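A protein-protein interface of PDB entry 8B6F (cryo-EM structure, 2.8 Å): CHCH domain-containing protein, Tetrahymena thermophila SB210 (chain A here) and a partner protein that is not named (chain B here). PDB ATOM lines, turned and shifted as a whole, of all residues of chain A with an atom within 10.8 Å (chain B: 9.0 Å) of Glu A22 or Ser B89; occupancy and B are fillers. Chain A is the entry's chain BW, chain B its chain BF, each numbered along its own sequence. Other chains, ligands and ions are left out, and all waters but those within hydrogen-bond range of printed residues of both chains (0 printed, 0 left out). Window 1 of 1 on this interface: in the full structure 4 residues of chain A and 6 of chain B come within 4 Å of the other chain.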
ATOM      1  N   TYR A  16       7.500   7.226  17.740  1.00  0.00           N
ATOM      2  CA  TYR A  16       7.653   8.585  18.236  1.00  0.00           C
ATOM      3  C   TYR A  16       6.927   8.756  19.564  1.00  0.00           C
ATOM      4  O   TYR A  16       5.835   8.220  19.766  1.00  0.00           O
ATOM      5  CB  TYR A  16       7.121   9.589  17.214  1.00  0.00           C
ATOM      6  CG  TYR A  16       7.884   9.590  15.909  1.00  0.00           C
ATOM      7  CD1 TYR A  16       7.584   8.679  14.905  1.00  0.00           C
ATOM      8  CD2 TYR A  16       8.901  10.505  15.680  1.00  0.00           C
ATOM      9  CE1 TYR A  16       8.278   8.678  13.711  1.00  0.00           C
ATOM     10  CE2 TYR A  16       9.604  10.511  14.490  1.00  0.00           C
ATOM     11  CZ  TYR A  16       9.286   9.596  13.510  1.00  0.00           C
ATOM     12  OH  TYR A  16       9.982   9.602  12.324  1.00  0.00           O
ATOM     13  N   SER A  17       7.544   9.510  20.469  1.00  0.00           N
ATOM     14  CA  SER A  17       6.974   9.751  21.784  1.00  0.00           C
ATOM     15  C   SER A  17       5.957  10.889  21.728  1.00  0.00           C
ATOM     16  O   SER A  17       5.769  11.547  20.703  1.00  0.00           O
ATOM     17  CB  SER A  17       8.075  10.066  22.794  1.00  0.00           C
ATOM     18  OG  SER A  17       8.832  11.193  22.389  1.00  0.00           O
ATOM     19  N   LYS A  18       5.294  11.121  22.864  1.00  0.00           N
ATOM     20  CA  LYS A  18       4.289  12.177  22.932  1.00  0.00           C
ATOM     21  C   LYS A  18       4.908  13.548  22.698  1.00  0.00           C
ATOM     22  O   LYS A  18       4.323  14.390  22.008  1.00  0.00           O
ATOM     23  CB  LYS A  18       3.573  12.130  24.281  1.00  0.00           C
ATOM     24  CG  LYS A  18       2.770  10.854  24.501  1.00  0.00           C
ATOM     25  CD  LYS A  18       2.208  10.773  25.914  1.00  0.00           C
ATOM     26  CE  LYS A  18       1.154  11.837  26.180  1.00  0.00           C
ATOM     27  NZ  LYS A  18      -0.017  11.705  25.269  1.00  0.00           N
ATOM     28  N   GLU A  19       6.092  13.792  23.259  1.00  0.00           N
ATOM     29  CA  GLU A  19       6.758  15.070  23.031  1.00  0.00           C
ATOM     30  C   GLU A  19       7.088  15.256  21.555  1.00  0.00           C
ATOM     31  O   GLU A  19       6.934  16.355  21.011  1.00  0.00           O
ATOM     32  CB  GLU A  19       8.028  15.167  23.877  1.00  0.00           C
ATOM     33  CG  GLU A  19       7.780  15.334  25.368  1.00  0.00           C
ATOM     34  CD  GLU A  19       7.303  14.060  26.033  1.00  0.00           C
ATOM     35  OE1 GLU A  19       7.329  13.000  25.376  1.00  0.00           O
ATOM     36  OE2 GLU A  19       6.903  14.119  27.213  1.00  0.00           O
ATOM     37  N   GLU A  20       7.550  14.195  20.892  1.00  0.00           N
ATOM     38  CA  GLU A  20       7.850  14.289  19.467  1.00  0.00           C
ATOM     39  C   GLU A  20       6.590  14.538  18.650  1.00  0.00           C
ATOM     40  O   GLU A  20       6.617  15.297  17.675  1.00  0.00           O
ATOM     41  CB  GLU A  20       8.557  13.019  18.996  1.00  0.00           C
ATOM     42  CG  GLU A  20       9.988  12.902  19.488  1.00  0.00           C
ATOM     43  CD  GLU A  20      10.662  11.634  19.014  1.00  0.00           C
ATOM     44  OE1 GLU A  20       9.969  10.771  18.440  1.00  0.00           O
ATOM     45  OE2 GLU A  20      11.885  11.497  19.214  1.00  0.00           O
ATOM     46  N   ILE A  21       5.475  13.906  19.024  1.00  0.00           N
ATOM     47  CA  ILE A  21       4.218  14.154  18.324  1.00  0.00           C
ATOM     48  C   ILE A  21       3.808  15.610  18.491  1.00  0.00           C
ATOM     49  O   ILE A  21       3.412  16.277  17.529  1.00  0.00           O
ATOM     50  CB  ILE A  21       3.123  13.196  18.828  1.00  0.00           C
ATOM     51  CG1 ILE A  21       3.478  11.753  18.470  1.00  0.00           C
ATOM     52  CG2 ILE A  21       1.766  13.568  18.235  1.00  0.00           C
ATOM     53  CD1 ILE A  21       2.625  10.719  19.169  1.00  0.00           C
ATOM     54  N   GLU A  22       3.902  16.126  19.717  1.00  0.00           N
ATOM     55  CA  GLU A  22       3.561  17.524  19.962  1.00  0.00           C
ATOM     56  C   GLU A  22       4.458  18.454  19.157  1.00  0.00           C
ATOM     57  O   GLU A  22       3.987  19.449  18.594  1.00  0.00           O
ATOM     58  CB  GLU A  22       3.667  17.834  21.454  1.00  0.00           C
ATOM     59  CG  GLU A  22       2.667  17.072  22.308  1.00  0.00           C
ATOM     60  CD  GLU A  22       2.984  17.155  23.788  1.00  0.00           C
ATOM     61  OE1 GLU A  22       3.966  17.836  24.150  1.00  0.00           O
ATOM     62  OE2 GLU A  22       2.252  16.538  24.589  1.00  0.00           O
ATOM     63  N   ALA A  23       5.755  18.151  19.094  1.00  0.00           N
ATOM     64  CA  ALA A  23       6.662  18.944  18.272  1.00  0.00           C
ATOM     65  C   ALA A  23       6.222  18.925  16.815  1.00  0.00           C
ATOM     66  O   ALA A  23       5.848  19.957  16.251  1.00  0.00           O
ATOM     67  CB  ALA A  23       8.090  18.417  18.415  1.00  0.00           C
ATOM     68  N   TYR A  24       6.241  17.747  16.191  1.00  0.00           N
ATOM     69  CA  TYR A  24       5.723  17.582  14.834  1.00  0.00           C
ATOM     70  C   TYR A  24       4.202  17.432  14.897  1.00  0.00           C
ATOM     71  O   TYR A  24       3.622  16.467  14.402  1.00  0.00           O
ATOM     72  CB  TYR A  24       6.352  16.371  14.158  1.00  0.00           C
ATOM     73  CG  TYR A  24       7.820  16.162  14.443  1.00  0.00           C
ATOM     74  CD1 TYR A  24       8.777  17.048  13.970  1.00  0.00           C
ATOM     75  CD2 TYR A  24       8.249  15.056  15.163  1.00  0.00           C
ATOM     76  CE1 TYR A  24      10.119  16.848  14.223  1.00  0.00           C
ATOM     77  CE2 TYR A  24       9.587  14.846  15.420  1.00  0.00           C
ATOM     78  CZ  TYR A  24      10.518  15.745  14.947  1.00  0.00           C
ATOM     79  OH  TYR A  24      11.853  15.537  15.201  1.00  0.00           O
ATOM     80  N   GLN A  25       3.561  18.417  15.528  1.00  0.00           N
ATOM     81  CA  GLN A  25       2.143  18.346  15.864  1.00  0.00           C
ATOM     82  C   GLN A  25       1.337  17.680  14.762  1.00  0.00           C
ATOM     83  O   GLN A  25       1.370  18.100  13.601  1.00  0.00           O
ATOM     84  CB  GLN A  25       1.599  19.753  16.147  1.00  0.00           C
ATOM     85  CG  GLN A  25       1.564  20.714  14.964  1.00  0.00           C
ATOM     86  CD  GLN A  25       2.939  21.073  14.447  1.00  0.00           C
ATOM     87  OE1 GLN A  25       3.727  20.199  14.091  1.00  0.00           O
ATOM     88  NE2 GLN A  25       3.241  22.367  14.412  1.00  0.00           N
ATOM     89  N   VAL A  26       0.622  16.629  15.134  1.00  0.00           N
ATOM     90  CA  VAL A  26      -0.162  15.813  14.212  1.00  0.00           C
ATOM     91  C   VAL A  26      -1.632  16.133  14.442  1.00  0.00           C
ATOM     92  O   VAL A  26      -2.061  16.210  15.598  1.00  0.00           O
ATOM     93  CB  VAL A  26       0.103  14.309  14.418  1.00  0.00           C
ATOM     94  CG1 VAL A  26      -0.717  13.474  13.449  1.00  0.00           C
ATOM     95  CG2 VAL A  26       1.584  14.005  14.268  1.00  0.00           C
ATOM     96  N   PRO A  27      -2.430  16.333  13.393  1.00  0.00           N
ATOM     97  CA  PRO A  27      -3.857  16.585  13.610  1.00  0.00           C
ATOM     98  C   PRO A  27      -4.515  15.410  14.316  1.00  0.00           C
ATOM     99  O   PRO A  27      -4.131  14.253  14.132  1.00  0.00           O
ATOM    100  CB  PRO A  27      -4.409  16.775  12.191  1.00  0.00           C
ATOM    101  CG  PRO A  27      -3.420  16.117  11.303  1.00  0.00           C
ATOM    102  CD  PRO A  27      -2.092  16.311  11.960  1.00  0.00           C
ATOM    103  N   MET A  28      -5.515  15.722  15.142  1.00  0.00           N
ATOM    104  CA  MET A  28      -6.191  14.675  15.898  1.00  0.00           C
ATOM    105  C   MET A  28      -6.766  13.609  14.977  1.00  0.00           C
ATOM    106  O   MET A  28      -6.845  12.437  15.360  1.00  0.00           O
ATOM    107  CB  MET A  28      -7.299  15.279  16.760  1.00  0.00           C
ATOM    108  CG  MET A  28      -7.904  14.308  17.761  1.00  0.00           C
ATOM    109  SD  MET A  28      -6.717  13.734  18.988  1.00  0.00           S
ATOM    110  CE  MET A  28      -7.724  12.581  19.914  1.00  0.00           C
ATOM    111  N   ARG A  29      -7.171  13.993  13.766  1.00  0.00           N
ATOM    112  CA  ARG A  29      -7.727  13.021  12.832  1.00  0.00           C
ATOM    113  C   ARG A  29      -6.748  11.884  12.581  1.00  0.00           C
ATOM    114  O   ARG A  29      -7.141  10.713  12.542  1.00  0.00           O
ATOM    115  CB  ARG A  29      -8.094  13.711  11.518  1.00  0.00           C
ATOM    116  CG  ARG A  29      -9.064  12.922  10.656  1.00  0.00           C
ATOM    117  CD  ARG A  29     -10.480  13.030  11.198  1.00  0.00           C
ATOM    118  NE  ARG A  29     -11.407  12.150  10.499  1.00  0.00           N
ATOM    119  CZ  ARG A  29     -12.713  12.109  10.725  1.00  0.00           C
ATOM    120  NH1 ARG A  29     -13.286  12.900  11.615  1.00  0.00           N
ATOM    121  NH2 ARG A  29     -13.462  11.249  10.041  1.00  0.00           N
ATOM    122  N   LYS A  31      -3.883  11.384  14.553  1.00  0.00           N
ATOM    123  CA  LYS A  31      -3.410  10.873  15.834  1.00  0.00           C
ATOM    124  C   LYS A  31      -4.347   9.812  16.396  1.00  0.00           C
ATOM    125  O   LYS A  31      -3.908   8.925  17.136  1.00  0.00           O
ATOM    126  CB  LYS A  31      -3.248  12.025  16.827  1.00  0.00           C
ATOM    127  CG  LYS A  31      -2.600  11.629  18.148  1.00  0.00           C
ATOM    128  CD  LYS A  31      -3.639  11.311  19.213  1.00  0.00           C
ATOM    129  CE  LYS A  31      -2.980  10.959  20.536  1.00  0.00           C
ATOM    130  NZ  LYS A  31      -3.985  10.638  21.588  1.00  0.00           N
ATOM    131  N   ALA A  32      -5.638   9.887  16.067  1.00  0.00           N
ATOM    132  CA  ALA A  32      -6.579   8.879  16.540  1.00  0.00           C
ATOM    133  C   ALA A  32      -6.258   7.507  15.962  1.00  0.00           C
ATOM    134  O   ALA A  32      -6.365   6.492  16.658  1.00  0.00           O
ATOM    135  CB  ALA A  32      -8.007   9.288  16.184  1.00  0.00           C
ATOM    136  N   VAL A  36       0.440   7.010  13.033  1.00  0.00           N
ATOM    137  CA  VAL A  36       1.236   8.167  13.424  1.00  0.00           C
ATOM    138  C   VAL A  36       2.702   7.943  13.079  1.00  0.00           C
ATOM    139  O   VAL A  36       3.391   8.856  12.609  1.00  0.00           O
ATOM    140  CB  VAL A  36       1.045   8.468  14.922  1.00  0.00           C
ATOM    141  CG1 VAL A  36       1.883   9.665  15.342  1.00  0.00           C
ATOM    142  CG2 VAL A  36      -0.421   8.711  15.229  1.00  0.00           C
ATOM    143  N   TYR A  39       3.050   8.459   9.479  1.00  0.00           N
ATOM    144  CA  TYR A  39       2.670   9.807   9.075  1.00  0.00           C
ATOM    145  C   TYR A  39       3.767  10.821   9.375  1.00  0.00           C
ATOM    146  O   TYR A  39       4.051  11.693   8.546  1.00  0.00           O
ATOM    147  CB  TYR A  39       1.372  10.209   9.778  1.00  0.00           C
ATOM    148  CG  TYR A  39       0.918  11.624   9.492  1.00  0.00           C
ATOM    149  CD1 TYR A  39       0.178  11.921   8.355  1.00  0.00           C
ATOM    150  CD2 TYR A  39       1.215  12.658  10.369  1.00  0.00           C
ATOM    151  CE1 TYR A  39      -0.244  13.209   8.094  1.00  0.00           C
ATOM    152  CE2 TYR A  39       0.798  13.950  10.117  1.00  0.00           C
ATOM    153  CZ  TYR A  39       0.067  14.218   8.978  1.00  0.00           C
ATOM    154  OH  TYR A  39      -0.351  15.501   8.720  1.00  0.00           O
ATOM    155  N   ILE A  40       4.396  10.722  10.548  1.00  0.00           N
ATOM    156  CA  ILE A  40       5.357  11.746  10.960  1.00  0.00           C
ATOM    157  C   ILE A  40       6.507  11.877   9.968  1.00  0.00           C
ATOM    158  O   ILE A  40       6.852  13.012   9.603  1.00  0.00           O
ATOM    159  CB  ILE A  40       5.838  11.469  12.395  1.00  0.00           C
ATOM    160  CG1 ILE A  40       4.711  11.768  13.386  1.00  0.00           C
ATOM    161  CG2 ILE A  40       7.078  12.300  12.722  1.00  0.00           C
ATOM    162  CD1 ILE A  40       5.008  11.352  14.809  1.00  0.00           C
ATOM    163  N   LYS A  43       5.280  13.927   7.031  1.00  0.00           N
ATOM    164  CA  LYS A  43       5.131  15.343   7.353  1.00  0.00           C
ATOM    165  C   LYS A  43       6.488  16.029   7.448  1.00  0.00           C
ATOM    166  O   LYS A  43       6.655  17.160   6.978  1.00  0.00           O
ATOM    167  CB  LYS A  43       4.356  15.507   8.661  1.00  0.00           C
ATOM    168  CG  LYS A  43       4.044  16.957   9.011  1.00  0.00           C
ATOM    169  CD  LYS A  43       3.312  17.061  10.337  1.00  0.00           C
ATOM    170  CE  LYS A  43       2.973  18.503  10.668  1.00  0.00           C
ATOM    171  NZ  LYS A  43       2.022  19.094   9.690  1.00  0.00           N
ATOM    172  N   LYS A  44       7.472  15.358   8.049  1.00  0.00           N
ATOM    173  CA  LYS A  44       8.812  15.928   8.130  1.00  0.00           C
ATOM    174  C   LYS A  44       9.404  16.127   6.742  1.00  0.00           C
ATOM    175  O   LYS A  44      10.026  17.158   6.467  1.00  0.00           O
ATOM    176  CB  LYS A  44       9.718  15.032   8.974  1.00  0.00           C
ATOM    177  CG  LYS A  44       9.354  14.996  10.449  1.00  0.00           C
ATOM    178  CD  LYS A  44      10.090  13.883  11.185  1.00  0.00           C
ATOM    179  CE  LYS A  44      11.598  14.079  11.169  1.00  0.00           C
ATOM    180  NZ  LYS A  44      12.009  15.348  11.827  1.00  0.00           N
ATOM    181  N   GLN A  47       7.756  19.137   5.177  1.00  0.00           N
ATOM    182  CA  GLN A  47       8.286  20.361   5.768  1.00  0.00           C
ATOM    183  C   GLN A  47       9.669  20.680   5.216  1.00  0.00           C
ATOM    184  O   GLN A  47       9.975  21.840   4.918  1.00  0.00           O
ATOM    185  CB  GLN A  47       8.334  20.224   7.288  1.00  0.00           C
ATOM    186  CG  GLN A  47       6.970  20.271   7.956  1.00  0.00           C
ATOM    187  CD  GLN A  47       6.445  21.683   8.111  1.00  0.00           C
ATOM    188  OE1 GLN A  47       7.205  22.649   8.068  1.00  0.00           O
ATOM    189  NE2 GLN A  47       5.136  21.809   8.294  1.00  0.00           N
ATOM    190  N   ALA B  81      -2.967  26.140  28.931  1.00  0.00           N
ATOM    191  CA  ALA B  81      -2.731  24.765  28.509  1.00  0.00           C
ATOM    192  C   ALA B  81      -3.301  24.511  27.122  1.00  0.00           C
ATOM    193  O   ALA B  81      -2.661  23.858  26.290  1.00  0.00           O
ATOM    194  CB  ALA B  81      -3.340  23.797  29.521  1.00  0.00           C
ATOM    195  N   LEU B  84      -0.939  26.271  24.542  1.00  0.00           N
ATOM    196  CA  LEU B  84       0.410  25.724  24.435  1.00  0.00           C
ATOM    197  C   LEU B  84       0.390  24.292  23.909  1.00  0.00           C
ATOM    198  O   LEU B  84       1.164  23.941  23.010  1.00  0.00           O
ATOM    199  CB  LEU B  84       1.108  25.782  25.794  1.00  0.00           C
ATOM    200  CG  LEU B  84       1.418  27.177  26.345  1.00  0.00           C
ATOM    201  CD1 LEU B  84       1.988  27.076  27.747  1.00  0.00           C
ATOM    202  CD2 LEU B  84       2.374  27.931  25.435  1.00  0.00           C
ATOM    203  N   THR B  85      -0.487  23.450  24.455  1.00  0.00           N
ATOM    204  CA  THR B  85      -0.460  22.022  24.148  1.00  0.00           C
ATOM    205  C   THR B  85      -1.429  21.706  23.014  1.00  0.00           C
ATOM    206  O   THR B  85      -2.574  22.168  23.042  1.00  0.00           O
ATOM    207  CB  THR B  85      -0.826  21.197  25.374  1.00  0.00           C
ATOM    208  OG1 THR B  85       0.045  21.529  26.460  1.00  0.00           O
ATOM    209  CG2 THR B  85      -0.709  19.707  25.081  1.00  0.00           C
ATOM    210  N   PRO B  86      -1.025  20.927  22.010  1.00  0.00           N
ATOM    211  CA  PRO B  86      -1.967  20.549  20.952  1.00  0.00           C
ATOM    212  C   PRO B  86      -3.061  19.641  21.493  1.00  0.00           C
ATOM    213  O   PRO B  86      -2.930  19.022  22.549  1.00  0.00           O
ATOM    214  CB  PRO B  86      -1.088  19.822  19.929  1.00  0.00           C
ATOM    215  CG  PRO B  86       0.067  19.324  20.715  1.00  0.00           C
ATOM    216  CD  PRO B  86       0.311  20.345  21.786  1.00  0.00           C
ATOM    217  N   THR B  87      -4.162  19.569  20.740  1.00  0.00           N
ATOM    218  CA  THR B  87      -5.323  18.823  21.212  1.00  0.00           C
ATOM    219  C   THR B  87      -4.962  17.384  21.556  1.00  0.00           C
ATOM    220  O   THR B  87      -5.577  16.787  22.447  1.00  0.00           O
ATOM    221  CB  THR B  87      -6.438  18.860  20.165  1.00  0.00           C
ATOM    222  OG1 THR B  87      -7.687  18.528  20.783  1.00  0.00           O
ATOM    223  CG2 THR B  87      -6.178  17.863  19.042  1.00  0.00           C
ATOM    224  N   SER B  88      -3.981  16.812  20.865  1.00  0.00           N
ATOM    225  CA  SER B  88      -3.484  15.495  21.233  1.00  0.00           C
ATOM    226  C   SER B  88      -2.673  15.599  22.516  1.00  0.00           C
ATOM    227  O   SER B  88      -1.772  16.433  22.628  1.00  0.00           O
ATOM    228  CB  SER B  88      -2.633  14.912  20.105  1.00  0.00           C
ATOM    229  OG  SER B  88      -1.500  15.723  19.850  1.00  0.00           O
ATOM    230  N   SER B  89      -2.997  14.751  23.488  1.00  0.00           N
ATOM    231  CA  SER B  89      -2.392  14.712  24.813  1.00  0.00           C
ATOM    232  C   SER B  89      -2.894  15.850  25.696  1.00  0.00           C
ATOM    233  O   SER B  89      -2.512  15.906  26.869  1.00  0.00           O
ATOM    234  CB  SER B  89      -0.857  14.764  24.766  1.00  0.00           C
ATOM    235  OG  SER B  89      -0.402  16.016  24.284  1.00  0.00           O
ATOM    236  N   LEU B  90      -3.717  16.765  25.180  1.00  0.00           N
ATOM    237  CA  LEU B  90      -4.211  17.858  26.010  1.00  0.00           C
ATOM    238  C   LEU B  90      -5.084  17.334  27.143  1.00  0.00           C
ATOM    239  O   LEU B  90      -4.898  17.705  28.307  1.00  0.00           O
ATOM    240  CB  LEU B  90      -4.982  18.862  25.153  1.00  0.00           C
ATOM    241  CG  LEU B  90      -5.650  20.016  25.909  1.00  0.00           C
ATOM    242  CD1 LEU B  90      -4.667  20.726  26.822  1.00  0.00           C
ATOM    243  CD2 LEU B  90      -6.264  20.999  24.930  1.00  0.00           C
ATOM    244  N   ARG B  91      -6.050  16.467  26.823  1.00  0.00           N
ATOM    245  CA  ARG B  91      -6.883  15.889  27.873  1.00  0.00           C
ATOM    246  C   ARG B  91      -6.090  14.941  28.758  1.00  0.00           C
ATOM    247  O   ARG B  91      -6.372  14.834  29.957  1.00  0.00           O
ATOM    248  CB  ARG B  91      -8.083  15.164  27.269  1.00  0.00           C
ATOM    249  CG  ARG B  91      -9.185  16.096  26.804  1.00  0.00           C
ATOM    250  CD  ARG B  91     -10.535  15.401  26.799  1.00  0.00           C
ATOM    251  NE  ARG B  91     -11.597  16.296  26.354  1.00  0.00           N
ATOM    252  CZ  ARG B  91     -12.880  15.968  26.292  1.00  0.00           C
ATOM    253  NH1 ARG B  91     -13.304  14.768  26.653  1.00  0.00           N
ATOM    254  NH2 ARG B  91     -13.758  16.863  25.847  1.00  0.00           N
ATOM    255  N   GLU B  92      -5.104  14.241  28.195  1.00  0.00           N
ATOM    256  CA  GLU B  92      -4.268  13.373  29.016  1.00  0.00           C
ATOM    257  C   GLU B  92      -3.538  14.179  30.080  1.00  0.00           C
ATOM    258  O   GLU B  92      -3.459  13.765  31.241  1.00  0.00           O
ATOM    259  CB  GLU B  92      -3.265  12.617  28.143  1.00  0.00           C
ATOM    260  CG  GLU B  92      -3.873  11.509  27.291  1.00  0.00           C
ATOM    261  CD  GLU B  92      -4.695  12.037  26.129  1.00  0.00           C
ATOM    262  OE1 GLU B  92      -4.871  13.268  26.027  1.00  0.00           O
ATOM    263  OE2 GLU B  92      -5.165  11.216  25.314  1.00  0.00           O
ATOM    264  N   LYS B  93      -3.001  15.340  29.701  1.00  0.00           N
ATOM    265  CA  LYS B  93      -2.305  16.187  30.659  1.00  0.00           C
ATOM    266  C   LYS B  93      -3.272  16.917  31.579  1.00  0.00           C
ATOM    267  O   LYS B  93      -2.910  17.248  32.713  1.00  0.00           O
ATOM    268  CB  LYS B  93      -1.419  17.186  29.917  1.00  0.00           C
ATOM    269  CG  LYS B  93      -0.314  16.529  29.103  1.00  0.00           C
ATOM    270  CD  LYS B  93       0.495  17.556  28.334  1.00  0.00           C
ATOM    271  CE  LYS B  93       1.608  16.894  27.542  1.00  0.00           C
ATOM    272  NZ  LYS B  93       2.423  17.891  26.796  1.00  0.00           N
ATOM    273  N   MET B  94      -4.497  17.182  31.118  1.00  0.00           N
ATOM    274  CA  MET B  94      -5.481  17.833  31.973  1.00  0.00           C
ATOM    275  C   MET B  94      -6.056  16.883  33.012  1.00  0.00           C
ATOM    276  O   MET B  94      -6.453  17.329  34.093  1.00  0.00           O
ATOM    277  CB  MET B  94      -6.616  18.421  31.135  1.00  0.00           C
ATOM    278  CG  MET B  94      -6.262  19.727  30.448  1.00  0.00           C
ATOM    279  SD  MET B  94      -7.678  20.507  29.648  1.00  0.00           S
ATOM    280  CE  MET B  94      -8.731  20.851  31.058  1.00  0.00           C
ATOM    281  N   ASN B  95      -6.110  15.585  32.718  1.00  0.00           N
ATOM    282  CA  ASN B  95      -6.608  14.622  33.692  1.00  0.00           C
ATOM    283  C   ASN B  95      -5.558  14.431  34.777  1.00  0.00           C
ATOM    284  O   ASN B  95      -4.997  13.343  34.941  1.00  0.00           O
ATOM    285  CB  ASN B  95      -6.946  13.293  33.020  1.00  0.00           C
ATOM    286  CG  ASN B  95      -8.053  13.426  31.998  1.00  0.00           C
ATOM    287  OD1 ASN B  95      -8.894  14.318  32.092  1.00  0.00           O
ATOM    288  ND2 ASN B  95      -8.058  12.538  31.012  1.00  0.00           N
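The side-chain hydroxyl of Ser B89 lies within hydrogen-bond range of the side-chain carboxylate of Glu A22 (2.7 Å).
OE2 of Glu B92 is in salt-bridge range of NZ of Lys A31, at 3.95 Å.
NZ of Lys B93 lies within salt-bridge range of OE2 of Glu A22 (2.6 Å).
The backbone NH (N) of Ser B89 sits close to the side-chain carboxylate (OE1) of Glu B92 (3.5 Å).
Lys A18 touches Ser B89.
Glu A22 touches Pro B86 (CG to CG, 3.8 Å).
CB of Met A28 touches CG2 of Thr B87 (3.6 Å).
CB of Ser B88 touches CG of Lys A31, 3.8 Å away.
Along chain A the printed residues that touch a printed residue of chain B span positions 18 to 31.
Hydrophobic or aromatic side chains of chain B within 4 Å of the printed part of chain A: Pro B86.
Along chain B the printed residues that touch a printed residue of chain A span positions 86 to 93.
Among the printed residues, 7 pairs touch across the chains.
Of chain B, only Pro B86 (3.8 Å), Ser B89 (2.7 Å) and Lys B93 (2.6 Å) come within 4 Å of Glu A22.
Printed residues of chain B within 4 Å of Met A28: Thr B87 (3.6 Å).
Printed residues of chain B within 4 Å of Lys A31: Ser B88 and Glu B92.
Of chain A, only Glu A22 (3.8 Å) comes within 4 Å of Pro B86.
Of chain A, only Lys A31 comes within 4 Å of Ser B88.
Of chain A, only Lys A18 and Glu A22 come within 4 Å of Ser B89.
Leu B90 touches none of the printed residues of chain A.
Of chain A, only Lys A31 comes within 4 Å of Glu B92.
Of chain A, only Glu A22 comes within 4 Å of Lys B93.
The nearest residue of chain B that does not touch Glu A22 is Thr B85 (4.4 Å).
The nearest printed residue of chain B that does not touch Met A28 is Ser B88 (4.3 Å).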
